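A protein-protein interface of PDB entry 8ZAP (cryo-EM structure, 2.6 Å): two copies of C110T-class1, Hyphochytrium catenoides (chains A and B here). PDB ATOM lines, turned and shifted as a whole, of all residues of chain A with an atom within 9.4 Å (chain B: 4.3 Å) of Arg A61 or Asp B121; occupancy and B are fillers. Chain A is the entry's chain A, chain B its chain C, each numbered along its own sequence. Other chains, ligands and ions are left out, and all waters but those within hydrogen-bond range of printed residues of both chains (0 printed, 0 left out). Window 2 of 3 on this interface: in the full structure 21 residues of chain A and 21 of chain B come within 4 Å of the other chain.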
ATOM      1  N   LEU A  46     -16.260   6.588  -9.366  1.00  0.00           N
ATOM      2  CA  LEU A  46     -15.516   5.417  -9.809  1.00  0.00           C
ATOM      3  C   LEU A  46     -16.010   4.934 -11.165  1.00  0.00           C
ATOM      4  O   LEU A  46     -15.209   4.583 -12.038  1.00  0.00           O
ATOM      5  CB  LEU A  46     -15.632   4.312  -8.762  1.00  0.00           C
ATOM      6  CG  LEU A  46     -14.956   2.990  -9.101  1.00  0.00           C
ATOM      7  CD1 LEU A  46     -13.452   3.146  -9.017  1.00  0.00           C
ATOM      8  CD2 LEU A  46     -15.446   1.899  -8.170  1.00  0.00           C
ATOM      9  N   ASP A  47     -17.327   4.914 -11.364  1.00  0.00           N
ATOM     10  CA  ASP A  47     -17.891   4.538 -12.653  1.00  0.00           C
ATOM     11  C   ASP A  47     -17.631   5.569 -13.741  1.00  0.00           C
ATOM     12  O   ASP A  47     -17.733   5.232 -14.925  1.00  0.00           O
ATOM     13  CB  ASP A  47     -19.397   4.307 -12.520  1.00  0.00           C
ATOM     14  CG  ASP A  47     -19.726   3.065 -11.724  1.00  0.00           C
ATOM     15  OD1 ASP A  47     -18.896   2.133 -11.706  1.00  0.00           O
ATOM     16  OD2 ASP A  47     -20.813   3.022 -11.112  1.00  0.00           O
ATOM     17  N   LEU A  48     -17.307   6.812 -13.374  1.00  0.00           N
ATOM     18  CA  LEU A  48     -17.018   7.832 -14.378  1.00  0.00           C
ATOM     19  C   LEU A  48     -15.776   7.493 -15.192  1.00  0.00           C
ATOM     20  O   LEU A  48     -15.750   7.730 -16.404  1.00  0.00           O
ATOM     21  CB  LEU A  48     -16.851   9.197 -13.711  1.00  0.00           C
ATOM     22  CG  LEU A  48     -18.113  10.018 -13.450  1.00  0.00           C
ATOM     23  CD1 LEU A  48     -17.753  11.473 -13.202  1.00  0.00           C
ATOM     24  CD2 LEU A  48     -19.093   9.897 -14.603  1.00  0.00           C
ATOM     25  N   GLY A  49     -14.742   6.954 -14.553  1.00  0.00           N
ATOM     26  CA  GLY A  49     -13.521   6.605 -15.251  1.00  0.00           C
ATOM     27  C   GLY A  49     -12.289   6.710 -14.380  1.00  0.00           C
ATOM     28  O   GLY A  49     -12.395   6.931 -13.170  1.00  0.00           O
ATOM     29  N   MET A  50     -11.113   6.554 -14.982  1.00  0.00           N
ATOM     30  CA  MET A  50      -9.851   6.626 -14.259  1.00  0.00           C
ATOM     31  C   MET A  50      -9.337   8.059 -14.237  1.00  0.00           C
ATOM     32  O   MET A  50      -9.314   8.734 -15.272  1.00  0.00           O
ATOM     33  CB  MET A  50      -8.808   5.709 -14.899  1.00  0.00           C
ATOM     34  CG  MET A  50      -8.856   4.273 -14.416  1.00  0.00           C
ATOM     35  SD  MET A  50      -8.068   3.121 -15.556  1.00  0.00           S
ATOM     36  CE  MET A  50      -8.437   3.890 -17.129  1.00  0.00           C
ATOM     37  N   LYS A  55     -10.742   8.764 -17.773  1.00  0.00           N
ATOM     38  CA  LYS A  55     -10.347   7.857 -18.840  1.00  0.00           C
ATOM     39  C   LYS A  55     -11.174   6.580 -18.758  1.00  0.00           C
ATOM     40  O   LYS A  55     -11.252   5.967 -17.687  1.00  0.00           O
ATOM     41  CB  LYS A  55      -8.858   7.535 -18.739  1.00  0.00           C
ATOM     42  CG  LYS A  55      -8.286   6.829 -19.953  1.00  0.00           C
ATOM     43  CD  LYS A  55      -6.808   6.543 -19.770  1.00  0.00           C
ATOM     44  CE  LYS A  55      -6.338   5.427 -20.687  1.00  0.00           C
ATOM     45  NZ  LYS A  55      -5.250   4.623 -20.071  1.00  0.00           N
ATOM     46  N   PRO A  56     -11.818   6.161 -19.846  1.00  0.00           N
ATOM     47  CA  PRO A  56     -12.638   4.945 -19.794  1.00  0.00           C
ATOM     48  C   PRO A  56     -11.804   3.721 -19.454  1.00  0.00           C
ATOM     49  O   PRO A  56     -10.653   3.593 -19.875  1.00  0.00           O
ATOM     50  CB  PRO A  56     -13.226   4.852 -21.207  1.00  0.00           C
ATOM     51  CG  PRO A  56     -12.345   5.704 -22.054  1.00  0.00           C
ATOM     52  CD  PRO A  56     -11.854   6.799 -21.172  1.00  0.00           C
ATOM     53  N   TYR A  57     -12.399   2.821 -18.679  1.00  0.00           N
ATOM     54  CA  TYR A  57     -11.739   1.566 -18.351  1.00  0.00           C
ATOM     55  C   TYR A  57     -11.636   0.690 -19.593  1.00  0.00           C
ATOM     56  O   TYR A  57     -12.519   0.701 -20.454  1.00  0.00           O
ATOM     57  CB  TYR A  57     -12.504   0.833 -17.251  1.00  0.00           C
ATOM     58  CG  TYR A  57     -12.523   1.563 -15.929  1.00  0.00           C
ATOM     59  CD1 TYR A  57     -11.484   1.420 -15.020  1.00  0.00           C
ATOM     60  CD2 TYR A  57     -13.582   2.393 -15.587  1.00  0.00           C
ATOM     61  CE1 TYR A  57     -11.497   2.084 -13.811  1.00  0.00           C
ATOM     62  CE2 TYR A  57     -13.605   3.061 -14.379  1.00  0.00           C
ATOM     63  CZ  TYR A  57     -12.558   2.903 -13.495  1.00  0.00           C
ATOM     64  OH  TYR A  57     -12.574   3.563 -12.290  1.00  0.00           O
ATOM     65  N   LYS A  58     -10.539  -0.065 -19.688  1.00  0.00           N
ATOM     66  CA  LYS A  58     -10.345  -0.934 -20.843  1.00  0.00           C
ATOM     67  C   LYS A  58     -11.427  -2.003 -20.920  1.00  0.00           C
ATOM     68  O   LYS A  58     -11.943  -2.295 -22.004  1.00  0.00           O
ATOM     69  CB  LYS A  58      -8.958  -1.573 -20.792  1.00  0.00           C
ATOM     70  CG  LYS A  58      -8.431  -2.016 -22.144  1.00  0.00           C
ATOM     71  CD  LYS A  58      -8.328  -0.843 -23.105  1.00  0.00           C
ATOM     72  CE  LYS A  58      -7.294  -1.104 -24.188  1.00  0.00           C
ATOM     73  NZ  LYS A  58      -5.911  -1.150 -23.640  1.00  0.00           N
ATOM     74  N   SER A  59     -11.788  -2.591 -19.781  1.00  0.00           N
ATOM     75  CA  SER A  59     -12.850  -3.587 -19.735  1.00  0.00           C
ATOM     76  C   SER A  59     -14.242  -2.972 -19.733  1.00  0.00           C
ATOM     77  O   SER A  59     -15.226  -3.709 -19.853  1.00  0.00           O
ATOM     78  CB  SER A  59     -12.687  -4.470 -18.497  1.00  0.00           C
ATOM     79  OG  SER A  59     -12.345  -3.695 -17.364  1.00  0.00           O
ATOM     80  N   GLY A  60     -14.349  -1.654 -19.601  1.00  0.00           N
ATOM     81  CA  GLY A  60     -15.630  -1.001 -19.459  1.00  0.00           C
ATOM     82  C   GLY A  60     -16.179  -0.993 -18.052  1.00  0.00           C
ATOM     83  O   GLY A  60     -17.260  -0.436 -17.829  1.00  0.00           O
ATOM     84  N   ARG A  61     -15.471  -1.590 -17.097  1.00  0.00           N
ATOM     85  CA  ARG A  61     -15.902  -1.635 -15.710  1.00  0.00           C
ATOM     86  C   ARG A  61     -14.704  -1.386 -14.809  1.00  0.00           C
ATOM     87  O   ARG A  61     -13.569  -1.736 -15.145  1.00  0.00           O
ATOM     88  CB  ARG A  61     -16.547  -2.983 -15.361  1.00  0.00           C
ATOM     89  CG  ARG A  61     -15.760  -4.184 -15.852  1.00  0.00           C
ATOM     90  CD  ARG A  61     -16.474  -5.489 -15.553  1.00  0.00           C
ATOM     91  NE  ARG A  61     -17.538  -5.768 -16.510  1.00  0.00           N
ATOM     92  CZ  ARG A  61     -18.176  -6.926 -16.599  1.00  0.00           C
ATOM     93  NH1 ARG A  61     -17.873  -7.944 -15.811  1.00  0.00           N
ATOM     94  NH2 ARG A  61     -19.139  -7.069 -17.504  1.00  0.00           N
ATOM     95  N   ALA A  62     -14.967  -0.774 -13.662  1.00  0.00           N
ATOM     96  CA  ALA A  62     -13.930  -0.501 -12.686  1.00  0.00           C
ATOM     97  C   ALA A  62     -13.528  -1.778 -11.959  1.00  0.00           C
ATOM     98  O   ALA A  62     -14.276  -2.760 -11.950  1.00  0.00           O
ATOM     99  CB  ALA A  62     -14.418   0.543 -11.688  1.00  0.00           C
ATOM    100  N   PRO A  63     -12.337  -1.805 -11.361  1.00  0.00           N
ATOM    101  CA  PRO A  63     -11.971  -2.943 -10.512  1.00  0.00           C
ATOM    102  C   PRO A  63     -12.949  -3.098  -9.356  1.00  0.00           C
ATOM    103  O   PRO A  63     -13.439  -2.116  -8.796  1.00  0.00           O
ATOM    104  CB  PRO A  63     -10.566  -2.582 -10.021  1.00  0.00           C
ATOM    105  CG  PRO A  63     -10.029  -1.677 -11.070  1.00  0.00           C
ATOM    106  CD  PRO A  63     -11.203  -0.886 -11.566  1.00  0.00           C
ATOM    107  N   GLU A  64     -13.236  -4.354  -9.008  1.00  0.00           N
ATOM    108  CA  GLU A  64     -14.245  -4.628  -7.990  1.00  0.00           C
ATOM    109  C   GLU A  64     -13.825  -4.122  -6.617  1.00  0.00           C
ATOM    110  O   GLU A  64     -14.666  -3.617  -5.865  1.00  0.00           O
ATOM    111  CB  GLU A  64     -14.542  -6.124  -7.936  1.00  0.00           C
ATOM    112  CG  GLU A  64     -14.895  -6.724  -9.280  1.00  0.00           C
ATOM    113  CD  GLU A  64     -16.376  -6.989  -9.421  1.00  0.00           C
ATOM    114  OE1 GLU A  64     -17.127  -6.668  -8.478  1.00  0.00           O
ATOM    115  OE2 GLU A  64     -16.792  -7.513 -10.476  1.00  0.00           O
ATOM    116  N   VAL A  65     -12.541  -4.249  -6.265  1.00  0.00           N
ATOM    117  CA  VAL A  65     -12.061  -3.772  -4.973  1.00  0.00           C
ATOM    118  C   VAL A  65     -12.101  -2.256  -4.865  1.00  0.00           C
ATOM    119  O   VAL A  65     -12.106  -1.724  -3.747  1.00  0.00           O
ATOM    120  CB  VAL A  65     -10.627  -4.265  -4.691  1.00  0.00           C
ATOM    121  CG1 VAL A  65     -10.646  -5.709  -4.225  1.00  0.00           C
ATOM    122  CG2 VAL A  65      -9.755  -4.099  -5.922  1.00  0.00           C
ATOM    123  N   ASN A  66     -12.133  -1.543  -5.988  1.00  0.00           N
ATOM    124  CA  ASN A  66     -12.230  -0.092  -5.978  1.00  0.00           C
ATOM    125  C   ASN A  66     -13.611   0.404  -5.578  1.00  0.00           C
ATOM    126  O   ASN A  66     -13.765   1.596  -5.288  1.00  0.00           O
ATOM    127  CB  ASN A  66     -11.863   0.473  -7.351  1.00  0.00           C
ATOM    128  CG  ASN A  66     -10.396   0.315  -7.671  1.00  0.00           C
ATOM    129  OD1 ASN A  66      -9.693  -0.474  -7.043  1.00  0.00           O
ATOM    130  ND2 ASN A  66      -9.922   1.069  -8.654  1.00  0.00           N
ATOM    131  N   SER A  67     -14.609  -0.472  -5.557  1.00  0.00           N
ATOM    132  CA  SER A  67     -15.934  -0.131  -5.064  1.00  0.00           C
ATOM    133  C   SER A  67     -16.051  -0.283  -3.557  1.00  0.00           C
ATOM    134  O   SER A  67     -17.124  -0.021  -3.007  1.00  0.00           O
ATOM    135  CB  SER A  67     -16.995  -1.001  -5.744  1.00  0.00           C
ATOM    136  OG  SER A  67     -16.718  -1.155  -7.123  1.00  0.00           O
ATOM    137  N   GLU A 247      -4.456   7.373 -10.562  1.00  0.00           N
ATOM    138  CA  GLU A 247      -4.842   6.971 -11.908  1.00  0.00           C
ATOM    139  C   GLU A 247      -4.476   8.031 -12.937  1.00  0.00           C
ATOM    140  O   GLU A 247      -4.105   7.693 -14.065  1.00  0.00           O
ATOM    141  CB  GLU A 247      -6.339   6.673 -11.962  1.00  0.00           C
ATOM    142  CG  GLU A 247      -6.760   5.463 -11.151  1.00  0.00           C
ATOM    143  CD  GLU A 247      -8.233   5.488 -10.796  1.00  0.00           C
ATOM    144  OE1 GLU A 247      -8.794   4.411 -10.508  1.00  0.00           O
ATOM    145  OE2 GLU A 247      -8.830   6.585 -10.806  1.00  0.00           O
ATOM    146  N   ALA B 117     -23.980 -13.224 -10.913  1.00  0.00           N
ATOM    147  CA  ALA B 117     -23.005 -12.282 -11.442  1.00  0.00           C
ATOM    148  C   ALA B 117     -21.793 -13.001 -12.009  1.00  0.00           C
ATOM    149  O   ALA B 117     -21.184 -12.522 -12.972  1.00  0.00           O
ATOM    150  CB  ALA B 117     -22.583 -11.296 -10.353  1.00  0.00           C
ATOM    151  N   PHE B 118     -21.436 -14.152 -11.440  1.00  0.00           N
ATOM    152  CA  PHE B 118     -20.315 -14.906 -11.977  1.00  0.00           C
ATOM    153  C   PHE B 118     -20.702 -15.661 -13.239  1.00  0.00           C
ATOM    154  O   PHE B 118     -19.854 -15.877 -14.111  1.00  0.00           O
ATOM    155  CB  PHE B 118     -19.773 -15.867 -10.921  1.00  0.00           C
ATOM    156  CG  PHE B 118     -18.756 -15.248 -10.011  1.00  0.00           C
ATOM    157  CD1 PHE B 118     -17.565 -14.757 -10.515  1.00  0.00           C
ATOM    158  CD2 PHE B 118     -18.993 -15.150  -8.652  1.00  0.00           C
ATOM    159  CE1 PHE B 118     -16.627 -14.183  -9.681  1.00  0.00           C
ATOM    160  CE2 PHE B 118     -18.058 -14.577  -7.812  1.00  0.00           C
ATOM    161  CZ  PHE B 118     -16.875 -14.094  -8.328  1.00  0.00           C
ATOM    162  N   THR B 119     -21.970 -16.058 -13.360  1.00  0.00           N
ATOM    163  CA  THR B 119     -22.390 -16.816 -14.531  1.00  0.00           C
ATOM    164  C   THR B 119     -22.552 -15.926 -15.754  1.00  0.00           C
ATOM    165  O   THR B 119     -22.255 -16.357 -16.873  1.00  0.00           O
ATOM    166  CB  THR B 119     -23.698 -17.553 -14.240  1.00  0.00           C
ATOM    167  OG1 THR B 119     -23.624 -18.161 -12.945  1.00  0.00           O
ATOM    168  CG2 THR B 119     -23.952 -18.627 -15.284  1.00  0.00           C
ATOM    169  N   LEU B 120     -23.009 -14.692 -15.561  1.00  0.00           N
ATOM    170  CA  LEU B 120     -23.266 -13.767 -16.655  1.00  0.00           C
ATOM    171  C   LEU B 120     -22.153 -12.745 -16.837  1.00  0.00           C
ATOM    172  O   LEU B 120     -22.279 -11.858 -17.688  1.00  0.00           O
ATOM    173  CB  LEU B 120     -24.600 -13.057 -16.433  1.00  0.00           C
ATOM    174  CG  LEU B 120     -25.806 -13.608 -17.189  1.00  0.00           C
ATOM    175  CD1 LEU B 120     -26.084 -15.039 -16.779  1.00  0.00           C
ATOM    176  CD2 LEU B 120     -27.019 -12.731 -16.931  1.00  0.00           C
ATOM    177  N   ASP B 121     -21.071 -12.851 -16.069  1.00  0.00           N
ATOM    178  CA  ASP B 121     -19.967 -11.893 -16.099  1.00  0.00           C
ATOM    179  C   ASP B 121     -20.480 -10.468 -15.894  1.00  0.00           C
ATOM    180  O   ASP B 121     -20.084  -9.522 -16.574  1.00  0.00           O
ATOM    181  CB  ASP B 121     -19.171 -12.012 -17.402  1.00  0.00           C
ATOM    182  CG  ASP B 121     -17.734 -11.557 -17.248  1.00  0.00           C
ATOM    183  OD1 ASP B 121     -17.279 -11.397 -16.097  1.00  0.00           O
ATOM    184  OD2 ASP B 121     -17.061 -11.356 -18.279  1.00  0.00           O
ATOM    185  N   LEU B 122     -21.389 -10.337 -14.935  1.00  0.00           N
ATOM    186  CA  LEU B 122     -22.022  -9.064 -14.622  1.00  0.00           C
ATOM    187  C   LEU B 122     -21.050  -8.151 -13.880  1.00  0.00           C
ATOM    188  O   LEU B 122     -20.284  -8.619 -13.034  1.00  0.00           O
ATOM    189  CB  LEU B 122     -23.269  -9.280 -13.774  1.00  0.00           C
ATOM    190  CG  LEU B 122     -24.416  -9.998 -14.483  1.00  0.00           C
ATOM    191  CD1 LEU B 122     -25.478 -10.432 -13.492  1.00  0.00           C
ATOM    192  CD2 LEU B 122     -25.014  -9.117 -15.564  1.00  0.00           C
ATOM    193  N   PRO B 123     -21.061  -6.859 -14.191  1.00  0.00           N
ATOM    194  CA  PRO B 123     -20.198  -5.921 -13.470  1.00  0.00           C
ATOM    195  C   PRO B 123     -20.694  -5.685 -12.052  1.00  0.00           C
ATOM    196  O   PRO B 123     -21.858  -5.923 -11.721  1.00  0.00           O
ATOM    197  CB  PRO B 123     -20.285  -4.642 -14.307  1.00  0.00           C
ATOM    198  CG  PRO B 123     -21.595  -4.742 -14.999  1.00  0.00           C
ATOM    199  CD  PRO B 123     -21.824  -6.198 -15.263  1.00  0.00           C
ATOM    200  N   LYS B 125     -19.941  -7.086  -9.012  1.00  0.00           N
ATOM    201  CA  LYS B 125     -20.394  -8.251  -8.260  1.00  0.00           C
ATOM    202  C   LYS B 125     -20.467  -7.953  -6.767  1.00  0.00           C
ATOM    203  O   LYS B 125     -21.421  -8.360  -6.092  1.00  0.00           O
ATOM    204  CB  LYS B 125     -19.469  -9.436  -8.532  1.00  0.00           C
ATOM    205  CG  LYS B 125     -19.288  -9.746 -10.007  1.00  0.00           C
ATOM    206  CD  LYS B 125     -18.605 -11.087 -10.210  1.00  0.00           C
ATOM    207  CE  LYS B 125     -18.463 -11.418 -11.684  1.00  0.00           C
ATOM    208  NZ  LYS B 125     -18.249 -10.204 -12.513  1.00  0.00           N
ATOM    209  N   ARG B 175     -25.993  -8.247 -21.118  1.00  0.00           N
ATOM    210  CA  ARG B 175     -25.400  -9.557 -21.346  1.00  0.00           C
ATOM    211  C   ARG B 175     -26.280 -10.433 -22.223  1.00  0.00           C
ATOM    212  O   ARG B 175     -25.768 -11.318 -22.917  1.00  0.00           O
ATOM    213  CB  ARG B 175     -25.129 -10.250 -20.012  1.00  0.00           C
ATOM    214  CG  ARG B 175     -24.157  -9.505 -19.117  1.00  0.00           C
ATOM    215  CD  ARG B 175     -22.788  -9.371 -19.762  1.00  0.00           C
ATOM    216  NE  ARG B 175     -22.172 -10.666 -20.021  1.00  0.00           N
ATOM    217  CZ  ARG B 175     -21.311 -10.902 -21.001  1.00  0.00           C
ATOM    218  NH1 ARG B 175     -20.943  -9.951 -21.842  1.00  0.00           N
ATOM    219  NH2 ARG B 175     -20.804 -12.123 -21.140  1.00  0.00           N
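NZ of Lys B125 is in salt-bridge range of OE2 of Glu A64. NH1 of Arg A61 lies within salt-bridge range of OD1 of Asp B121 (3.5 Å).
OD1 of Asp B121 is in salt-bridge range of NZ of Lys B125. The backbone carbonyl oxygen (O) of Ala B117 sits at hydrogen-bond distance from the backbone NH (N) of Leu B122, at 2.9 Å. The side-chain hydroxyl (OG) of Ser A67 lies within hydrogen-bond range of the backbone carbonyl oxygen (O) of Glu A64 (3.4 Å). The side-chain hydroxyl (OG) of Ser A59 sits at hydrogen-bond distance from the backbone carbonyl oxygen (O) of Arg A61 (3.2 Å). The backbone carbonyl oxygen of Leu B122 is in hydrogen-bond range of the side-chain amino group of Lys B125 (2.6 Å).
Among the printed residues, pairs that only touch across the chains: Arg A61 with Leu B122 (3.7 Å) and Arg A61 with Pro B123 (3.6 Å).
Asp B121 touches just one residue of chain A: Arg A61 (2.8 Å). Printed residues of chain A within 4 Å of Pro B123: Arg A61 (3.6 Å). Printed residues of chain A within 4 Å of Lys B125: Glu A64. The nearest printed residue of chain A that does not touch Lys B125 is Arg A61 (4.02 Å).
Printed residues of chain A that touch a printed residue of chain B: Arg A61 and Glu A64. Hydrophobic or aromatic side chains of chain B within 4 Å of the printed part of chain A: Pro B123. Along chain B the printed residues that touch a printed residue of chain A span positions 121 to 125. Among the printed residues, 4 pairs touch across the chains.
No position is printed for both chains.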
